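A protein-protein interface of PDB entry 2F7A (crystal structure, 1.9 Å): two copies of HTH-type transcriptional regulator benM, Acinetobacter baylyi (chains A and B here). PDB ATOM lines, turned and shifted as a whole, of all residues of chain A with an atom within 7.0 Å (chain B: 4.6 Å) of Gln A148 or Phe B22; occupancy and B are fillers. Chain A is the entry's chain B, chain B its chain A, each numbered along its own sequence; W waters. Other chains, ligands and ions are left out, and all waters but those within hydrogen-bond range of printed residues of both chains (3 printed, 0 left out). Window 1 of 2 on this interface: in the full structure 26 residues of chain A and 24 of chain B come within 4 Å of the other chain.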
ATOM      1  N   PHE A  22       5.781   8.613  25.927  1.00  0.00           N
ATOM      2  CA  PHE A  22       6.457   9.768  25.344  1.00  0.00           C
ATOM      3  C   PHE A  22       5.733  10.268  24.101  1.00  0.00           C
ATOM      4  O   PHE A  22       6.062  11.331  23.587  1.00  0.00           O
ATOM      5  CB  PHE A  22       7.921   9.427  25.034  1.00  0.00           C
ATOM      6  CG  PHE A  22       8.720   9.086  26.260  1.00  0.00           C
ATOM      7  CD1 PHE A  22       9.101  10.078  27.150  1.00  0.00           C
ATOM      8  CD2 PHE A  22       9.055   7.767  26.545  1.00  0.00           C
ATOM      9  CE1 PHE A  22       9.837   9.768  28.299  1.00  0.00           C
ATOM     10  CE2 PHE A  22       9.784   7.446  27.690  1.00  0.00           C
ATOM     11  CZ  PHE A  22      10.173   8.445  28.570  1.00  0.00           C
ATOM     12  N   TYR A 115      17.097  -1.799  22.858  1.00  0.00           N
ATOM     13  CA  TYR A 115      16.335  -1.923  24.097  1.00  0.00           C
ATOM     14  C   TYR A 115      15.006  -2.604  23.758  1.00  0.00           C
ATOM     15  O   TYR A 115      14.611  -2.636  22.587  1.00  0.00           O
ATOM     16  CB  TYR A 115      16.075  -0.533  24.700  1.00  0.00           C
ATOM     17  CG  TYR A 115      15.263   0.352  23.789  1.00  0.00           C
ATOM     18  CD1 TYR A 115      13.874   0.349  23.853  1.00  0.00           C
ATOM     19  CD2 TYR A 115      15.875   1.161  22.834  1.00  0.00           C
ATOM     20  CE1 TYR A 115      13.118   1.127  23.016  1.00  0.00           C
ATOM     21  CE2 TYR A 115      15.113   1.960  21.983  1.00  0.00           C
ATOM     22  CZ  TYR A 115      13.737   1.936  22.083  1.00  0.00           C
ATOM     23  OH  TYR A 115      12.960   2.694  21.245  1.00  0.00           O
ATOM     24  N   VAL A 144      20.102  -2.218  26.327  1.00  0.00           N
ATOM     25  CA  VAL A 144      19.901  -1.501  27.584  1.00  0.00           C
ATOM     26  C   VAL A 144      18.432  -1.564  28.016  1.00  0.00           C
ATOM     27  O   VAL A 144      17.575  -2.026  27.262  1.00  0.00           O
ATOM     28  CB  VAL A 144      20.416  -0.030  27.498  1.00  0.00           C
ATOM     29  CG1 VAL A 144      21.880  -0.016  27.064  1.00  0.00           C
ATOM     30  CG2 VAL A 144      19.557   0.829  26.554  1.00  0.00           C
ATOM     31  N   ARG A 145      18.162  -1.117  29.238  1.00  0.00           N
ATOM     32  CA  ARG A 145      16.862  -1.320  29.899  1.00  0.00           C
ATOM     33  C   ARG A 145      15.663  -0.701  29.194  1.00  0.00           C
ATOM     34  O   ARG A 145      14.599  -1.303  29.126  1.00  0.00           O
ATOM     35  CB  ARG A 145      16.889  -0.757  31.333  1.00  0.00           C
ATOM     36  CG  ARG A 145      17.239  -1.758  32.402  1.00  0.00           C
ATOM     37  CD  ARG A 145      17.028  -1.179  33.801  1.00  0.00           C
ATOM     38  NE  ARG A 145      15.643  -0.739  34.017  1.00  0.00           N
ATOM     39  CZ  ARG A 145      15.238   0.526  34.165  1.00  0.00           C
ATOM     40  NH1 ARG A 145      16.100   1.535  34.147  1.00  0.00           N
ATOM     41  NH2 ARG A 145      13.949   0.785  34.350  1.00  0.00           N
ATOM     42  N   GLU A 146      15.821   0.526  28.722  1.00  0.00           N
ATOM     43  CA  GLU A 146      14.684   1.277  28.230  1.00  0.00           C
ATOM     44  C   GLU A 146      15.134   2.397  27.296  1.00  0.00           C
ATOM     45  O   GLU A 146      16.329   2.724  27.222  1.00  0.00           O
ATOM     46  CB  GLU A 146      13.868   1.824  29.415  1.00  0.00           C
ATOM     47  CG  GLU A 146      14.671   2.722  30.362  1.00  0.00           C
ATOM     48  CD  GLU A 146      13.957   3.026  31.681  1.00  0.00           C
ATOM     49  OE1 GLU A 146      12.919   2.398  31.989  1.00  0.00           O
ATOM     50  OE2 GLU A 146      14.447   3.907  32.420  1.00  0.00           O
ATOM     51  N   VAL A 147      14.168   2.963  26.575  1.00  0.00           N
ATOM     52  CA  VAL A 147      14.459   3.968  25.560  1.00  0.00           C
ATOM     53  C   VAL A 147      15.120   5.229  26.122  1.00  0.00           C
ATOM     54  O   VAL A 147      16.020   5.781  25.486  1.00  0.00           O
ATOM     55  CB  VAL A 147      13.196   4.362  24.741  1.00  0.00           C
ATOM     56  CG1 VAL A 147      12.159   5.077  25.608  1.00  0.00           C
ATOM     57  CG2 VAL A 147      13.596   5.219  23.536  1.00  0.00           C
ATOM     58  N   GLN A 148      14.685   5.698  27.293  1.00  0.00           N
ATOM     59  CA  GLN A 148      15.244   6.946  27.846  1.00  0.00           C
ATOM     60  C   GLN A 148      16.725   6.771  28.218  1.00  0.00           C
ATOM     61  O   GLN A 148      17.517   7.709  28.103  1.00  0.00           O
ATOM     62  CB  GLN A 148      14.419   7.479  29.034  1.00  0.00           C
ATOM     63  CG  GLN A 148      14.685   6.791  30.375  1.00  0.00           C
ATOM     64  CD  GLN A 148      13.474   6.805  31.298  1.00  0.00           C
ATOM     65  OE1 GLN A 148      12.429   6.242  30.959  1.00  0.00           O
ATOM     66  NE2 GLN A 148      13.610   7.421  32.478  1.00  0.00           N
ATOM     67  N   LEU A 149      17.091   5.557  28.625  1.00  0.00           N
ATOM     68  CA  LEU A 149      18.479   5.211  28.927  1.00  0.00           C
ATOM     69  C   LEU A 149      19.312   5.158  27.655  1.00  0.00           C
ATOM     70  O   LEU A 149      20.425   5.675  27.618  1.00  0.00           O
ATOM     71  CB  LEU A 149      18.550   3.870  29.649  1.00  0.00           C
ATOM     72  CG  LEU A 149      19.929   3.286  29.984  1.00  0.00           C
ATOM     73  CD1 LEU A 149      20.789   4.250  30.791  1.00  0.00           C
ATOM     74  CD2 LEU A 149      19.758   1.956  30.732  1.00  0.00           C
ATOM     75  N   ALA A 150      18.770   4.543  26.611  1.00  0.00           N
ATOM     76  CA  ALA A 150      19.440   4.504  25.321  1.00  0.00           C
ATOM     77  C   ALA A 150      19.750   5.917  24.825  1.00  0.00           C
ATOM     78  O   ALA A 150      20.870   6.219  24.404  1.00  0.00           O
ATOM     79  CB  ALA A 150      18.584   3.752  24.308  1.00  0.00           C
ATOM     80  N   LEU A 151      18.751   6.787  24.910  1.00  0.00           N
ATOM     81  CA  LEU A 151      18.885   8.162  24.436  1.00  0.00           C
ATOM     82  C   LEU A 151      19.881   8.969  25.260  1.00  0.00           C
ATOM     83  O   LEU A 151      20.710   9.687  24.703  1.00  0.00           O
ATOM     84  CB  LEU A 151      17.519   8.846  24.418  1.00  0.00           C
ATOM     85  CG  LEU A 151      16.602   8.250  23.359  1.00  0.00           C
ATOM     86  CD1 LEU A 151      15.173   8.809  23.487  1.00  0.00           C
ATOM     87  CD2 LEU A 151      17.175   8.467  21.959  1.00  0.00           C
ATOM     88  N   GLY A 152      19.805   8.852  26.583  1.00  0.00           N
ATOM     89  CA  GLY A 152      20.778   9.502  27.458  1.00  0.00           C
ATOM     90  C   GLY A 152      22.197   9.032  27.184  1.00  0.00           C
ATOM     91  O   GLY A 152      23.142   9.818  27.231  1.00  0.00           O
ATOM     92  N   LEU A 153      22.351   7.746  26.891  1.00  0.00           N
ATOM     93  CA  LEU A 153      23.668   7.195  26.566  1.00  0.00           C
ATOM     94  C   LEU A 153      24.191   7.675  25.211  1.00  0.00           C
ATOM     95  O   LEU A 153      25.393   7.890  25.061  1.00  0.00           O
ATOM     96  CB  LEU A 153      23.632   5.672  26.612  1.00  0.00           C
ATOM     97  CG  LEU A 153      23.446   5.045  28.000  1.00  0.00           C
ATOM     98  CD1 LEU A 153      23.216   3.557  27.835  1.00  0.00           C
ATOM     99  CD2 LEU A 153      24.613   5.306  28.952  1.00  0.00           C
ATOM    100  N   VAL A 154      23.301   7.845  24.235  1.00  0.00           N
ATOM    101  CA  VAL A 154      23.667   8.460  22.937  1.00  0.00           C
ATOM    102  C   VAL A 154      24.195   9.881  23.165  1.00  0.00           C
ATOM    103  O   VAL A 154      25.227  10.275  22.612  1.00  0.00           O
ATOM    104  CB  VAL A 154      22.465   8.484  21.939  1.00  0.00           C
ATOM    105  CG1 VAL A 154      22.698   9.476  20.777  1.00  0.00           C
ATOM    106  CG2 VAL A 154      22.201   7.099  21.387  1.00  0.00           C
ATOM    107  N   ILE A 170      11.675  13.678  23.971  1.00  0.00           N
ATOM    108  CA  ILE A 170      12.893  13.683  24.759  1.00  0.00           C
ATOM    109  C   ILE A 170      13.937  14.512  24.015  1.00  0.00           C
ATOM    110  O   ILE A 170      14.549  14.050  23.044  1.00  0.00           O
ATOM    111  CB  ILE A 170      13.394  12.236  24.974  1.00  0.00           C
ATOM    112  CG1 ILE A 170      12.282  11.396  25.632  1.00  0.00           C
ATOM    113  CG2 ILE A 170      14.718  12.224  25.777  1.00  0.00           C
ATOM    114  CD1 ILE A 170      12.569   9.920  25.756  1.00  0.00           C
ATOM    115  N   GLN A 171      14.117  15.754  24.451  1.00  0.00           N
ATOM    116  CA  GLN A 171      15.071  16.654  23.816  1.00  0.00           C
ATOM    117  C   GLN A 171      16.263  16.897  24.731  1.00  0.00           C
ATOM    118  O   GLN A 171      16.294  17.853  25.514  1.00  0.00           O
ATOM    119  CB  GLN A 171      14.391  17.967  23.418  1.00  0.00           C
ATOM    120  CG  GLN A 171      13.401  17.800  22.261  1.00  0.00           C
ATOM    121  CD  GLN A 171      14.092  17.495  20.935  1.00  0.00           C
ATOM    122  OE1 GLN A 171      15.098  18.122  20.584  1.00  0.00           O
ATOM    123  NE2 GLN A 171      13.559  16.524  20.195  1.00  0.00           N
ATOM    124  N   LEU A 172      17.245  16.007  24.637  1.00  0.00           N
ATOM    125  CA  LEU A 172      18.454  16.129  25.440  1.00  0.00           C
ATOM    126  C   LEU A 172      19.456  17.010  24.714  1.00  0.00           C
ATOM    127  O   LEU A 172      19.469  17.064  23.489  1.00  0.00           O
ATOM    128  CB  LEU A 172      19.059  14.757  25.712  1.00  0.00           C
ATOM    129  CG  LEU A 172      18.098  13.711  26.300  1.00  0.00           C
ATOM    130  CD1 LEU A 172      18.833  12.435  26.640  1.00  0.00           C
ATOM    131  CD2 LEU A 172      17.366  14.256  27.526  1.00  0.00           C
ATOM    132  N   PHE A 173      20.283  17.701  25.493  1.00  0.00           N
ATOM    133  CA  PHE A 173      21.383  18.510  24.984  1.00  0.00           C
ATOM    134  C   PHE A 173      22.269  17.730  24.011  1.00  0.00           C
ATOM    135  O   PHE A 173      22.825  16.682  24.357  1.00  0.00           O
ATOM    136  CB  PHE A 173      22.234  19.000  26.159  1.00  0.00           C
ATOM    137  CG  PHE A 173      23.337  19.933  25.772  1.00  0.00           C
ATOM    138  CD1 PHE A 173      23.079  21.277  25.580  1.00  0.00           C
ATOM    139  CD2 PHE A 173      24.637  19.473  25.618  1.00  0.00           C
ATOM    140  CE1 PHE A 173      24.100  22.154  25.235  1.00  0.00           C
ATOM    141  CE2 PHE A 173      25.652  20.335  25.282  1.00  0.00           C
ATOM    142  CZ  PHE A 173      25.385  21.681  25.087  1.00  0.00           C
ATOM    143  N   SER B  19      17.743   9.348  36.238  1.00  0.00           N
ATOM    144  CA  SER B  19      17.143  10.657  35.967  1.00  0.00           C
ATOM    145  C   SER B  19      18.181  11.736  35.641  1.00  0.00           C
ATOM    146  O   SER B  19      17.866  12.731  34.979  1.00  0.00           O
ATOM    147  CB  SER B  19      16.305  11.099  37.164  1.00  0.00           C
ATOM    148  OG  SER B  19      17.102  11.152  38.333  1.00  0.00           O
ATOM    149  N   LEU B  20      19.415  11.531  36.091  1.00  0.00           N
ATOM    150  CA  LEU B  20      20.514  12.462  35.801  1.00  0.00           C
ATOM    151  C   LEU B  20      20.865  12.539  34.313  1.00  0.00           C
ATOM    152  O   LEU B  20      21.525  13.477  33.897  1.00  0.00           O
ATOM    153  CB  LEU B  20      21.765  12.104  36.613  1.00  0.00           C
ATOM    154  CG  LEU B  20      21.573  12.110  38.136  1.00  0.00           C
ATOM    155  CD1 LEU B  20      22.895  11.883  38.882  1.00  0.00           C
ATOM    156  CD2 LEU B  20      20.898  13.387  38.609  1.00  0.00           C
ATOM    157  N   LEU B  21      20.422  11.565  33.516  1.00  0.00           N
ATOM    158  CA  LEU B  21      20.593  11.627  32.062  1.00  0.00           C
ATOM    159  C   LEU B  21      19.779  12.739  31.391  1.00  0.00           C
ATOM    160  O   LEU B  21      20.041  13.085  30.236  1.00  0.00           O
ATOM    161  CB  LEU B  21      20.242  10.284  31.410  1.00  0.00           C
ATOM    162  CG  LEU B  21      21.162   9.090  31.705  1.00  0.00           C
ATOM    163  CD1 LEU B  21      20.572   7.825  31.084  1.00  0.00           C
ATOM    164  CD2 LEU B  21      22.574   9.315  31.221  1.00  0.00           C
ATOM    165  N   PHE B  22      18.790  13.285  32.104  1.00  0.00           N
ATOM    166  CA  PHE B  22      17.967  14.374  31.595  1.00  0.00           C
ATOM    167  C   PHE B  22      18.561  15.745  31.813  1.00  0.00           C
ATOM    168  O   PHE B  22      18.060  16.707  31.257  1.00  0.00           O
ATOM    169  CB  PHE B  22      16.586  14.364  32.264  1.00  0.00           C
ATOM    170  CG  PHE B  22      15.826  13.094  32.074  1.00  0.00           C
ATOM    171  CD1 PHE B  22      15.814  12.445  30.852  1.00  0.00           C
ATOM    172  CD2 PHE B  22      15.078  12.569  33.111  1.00  0.00           C
ATOM    173  CE1 PHE B  22      15.098  11.280  30.680  1.00  0.00           C
ATOM    174  CE2 PHE B  22      14.366  11.401  32.942  1.00  0.00           C
ATOM    175  CZ  PHE B  22      14.380  10.758  31.727  1.00  0.00           C
ATOM    176  N   GLY B  23      19.595  15.840  32.646  1.00  0.00           N
ATOM    177  CA  GLY B  23      20.241  17.112  32.939  1.00  0.00           C
ATOM    178  C   GLY B  23      21.624  17.192  32.313  1.00  0.00           C
ATOM    179  O   GLY B  23      21.792  16.898  31.136  1.00  0.00           O
ATOM    180  N   VAL B 147       9.479   7.786  37.075  1.00  0.00           N
ATOM    181  CA  VAL B 147       9.227   9.180  36.678  1.00  0.00           C
ATOM    182  C   VAL B 147       8.419   9.306  35.373  1.00  0.00           C
ATOM    183  O   VAL B 147       7.531  10.151  35.267  1.00  0.00           O
ATOM    184  CB  VAL B 147      10.542  10.016  36.579  1.00  0.00           C
ATOM    185  CG1 VAL B 147      11.480   9.500  35.484  1.00  0.00           C
ATOM    186  CG2 VAL B 147      10.220  11.489  36.360  1.00  0.00           C
ATOM    187  N   GLN B 148       8.716   8.456  34.397  1.00  0.00           N
ATOM    188  CA  GLN B 148       8.056   8.536  33.096  1.00  0.00           C
ATOM    189  C   GLN B 148       6.564   8.220  33.173  1.00  0.00           C
ATOM    190  O   GLN B 148       5.775   8.815  32.449  1.00  0.00           O
ATOM    191  CB  GLN B 148       8.771   7.672  32.031  1.00  0.00           C
ATOM    192  CG  GLN B 148       8.788   6.167  32.279  1.00  0.00           C
ATOM    193  CD  GLN B 148      10.061   5.670  32.970  1.00  0.00           C
ATOM    194  OE1 GLN B 148      10.677   6.382  33.774  1.00  0.00           O
ATOM    195  NE2 GLN B 148      10.453   4.435  32.661  1.00  0.00           N
ATOM    196  N   SER B 166      15.589  19.493  35.781  1.00  0.00           N
ATOM    197  CA  SER B 166      16.147  18.907  34.554  1.00  0.00           C
ATOM    198  C   SER B 166      15.133  18.040  33.790  1.00  0.00           C
ATOM    199  O   SER B 166      15.327  17.755  32.616  1.00  0.00           O
ATOM    200  CB  SER B 166      17.445  18.127  34.839  1.00  0.00           C
ATOM    201  OG  SER B 166      17.287  17.189  35.894  1.00  0.00           O
ATOM    202  N   SER B 169      13.582  18.503  30.033  1.00  0.00           N
ATOM    203  CA  SER B 169      14.096  17.916  28.797  1.00  0.00           C
ATOM    204  C   SER B 169      13.042  17.039  28.117  1.00  0.00           C
ATOM    205  O   SER B 169      13.090  16.800  26.908  1.00  0.00           O
ATOM    206  CB  SER B 169      15.437  17.207  29.051  1.00  0.00           C
ATOM    207  OG  SER B 169      16.485  18.158  29.200  1.00  0.00           O
ATOM    208  N   ILE B 170      12.100  16.552  28.916  1.00  0.00           N
ATOM    209  CA  ILE B 170      11.011  15.720  28.437  1.00  0.00           C
ATOM    210  C   ILE B 170       9.782  16.599  28.226  1.00  0.00           C
ATOM    211  O   ILE B 170       9.118  16.986  29.186  1.00  0.00           O
ATOM    212  CB  ILE B 170      10.675  14.604  29.444  1.00  0.00           C
ATOM    213  CG1 ILE B 170      11.927  13.759  29.731  1.00  0.00           C
ATOM    214  CG2 ILE B 170       9.506  13.750  28.923  1.00  0.00           C
ATOM    215  CD1 ILE B 170      11.741  12.750  30.854  1.00  0.00           C
HETATM  216  O   HOH W   1      11.677  18.075  24.966  1.00  0.00           O
HETATM  217  O   HOH W   2      19.371  17.807  28.159  1.00  0.00           O
HETATM  218  O   HOH W   3      12.921   4.872  34.609  1.00  0.00           O
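Water W1 bridges the backbone carbonyl oxygen (O) of Ser B169 (2.7 Å) and the backbone NH (N) of Gln A171 (3.4 Å).
Water W2 lies within hydrogen-bond range of N of Phe A173 (2.8 Å) and OG of Ser B169 (3.1 Å).
Water W3 lies within hydrogen-bond range of the side-chain amide oxygen (OE1) of Gln B148 (2.8 Å), the side-chain carboxylate (OE2) of Glu A146 (2.8 Å) and the side-chain amide nitrogen (NE2) of Gln A148 (3.4 Å).
Phe A22 touches Gln B148 (CZ to CB, 3.8 Å).
Gln A148 touches Phe B22 (NE2 to CZ, 3.5 Å).
CD1 of Leu A149 touches CD1 of Leu B21, at 3.6 Å.
C of Ile A170 touches O of Ser B169, 3.8 Å away.
Leu A172 touches Leu B21.
Leu A172 touches Ser B169.
Gln A148 touches two residues of chain B.
Of the printed residues of chain B, Leu A149 touches Leu B21.
Printed residues of chain B within 4 Å of Ile A170: Ser B169 (3.8 Å).
Phe A173 touches none of the printed residues of chain B.
Phe B22 touches one residue of chain A.
The nearest residue of chain B that does not touch Gln A148 is Val B147 (4.2 Å).
The nearest printed residue of chain A that does not touch Ser B169 is Phe A173 (5.3 Å).
Printed residues of chain A that touch a printed residue of chain B: Phe A22, Glu A146, Gln A148, Leu A149, Ile A170, Gln A171 and Leu A172.
Of the 10 printed residues of chain B, 4 touch a printed residue of chain A.
Hydrophobic or aromatic side chains of chain B that line the printed part of chain A: Leu B21 and Phe B22.
Among the printed residues, 9 pairs touch across the chains.
The side-chain amide oxygen (OE1) of Gln A148 sits close to the side-chain carboxylate (OE2) of Glu A146, 3.4 Å away.
The side-chain hydroxyl (OG) of Ser B169 sits at hydrogen-bond distance from the backbone carbonyl oxygen (O) of Phe B22 (3.0 Å).
The guanidinium group (NH2) of Arg A145 lies within salt-bridge range of the side-chain carboxylate (OE1) of Glu A146, 3.0 Å away.
Phe A22 touches Gln B148, and with the chains exchanged Gln A148 touches Phe B22.
Gln B148 touches its own counterpart, Gln A148.
Of the 9 pairs that touch across the chains among the printed residues, 3 have their exchanged pair printed and touching as well.
OE1 of Gln A148 lies close to NE2 of Gln B148 (3.2 Å).
NE2 of Gln B148 is in hydrogen-bond range of OE1 of Glu A146 (3.3 Å).
O of Ser B169 is in hydrogen-bond range of N of Gln A171 (2.9 Å).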
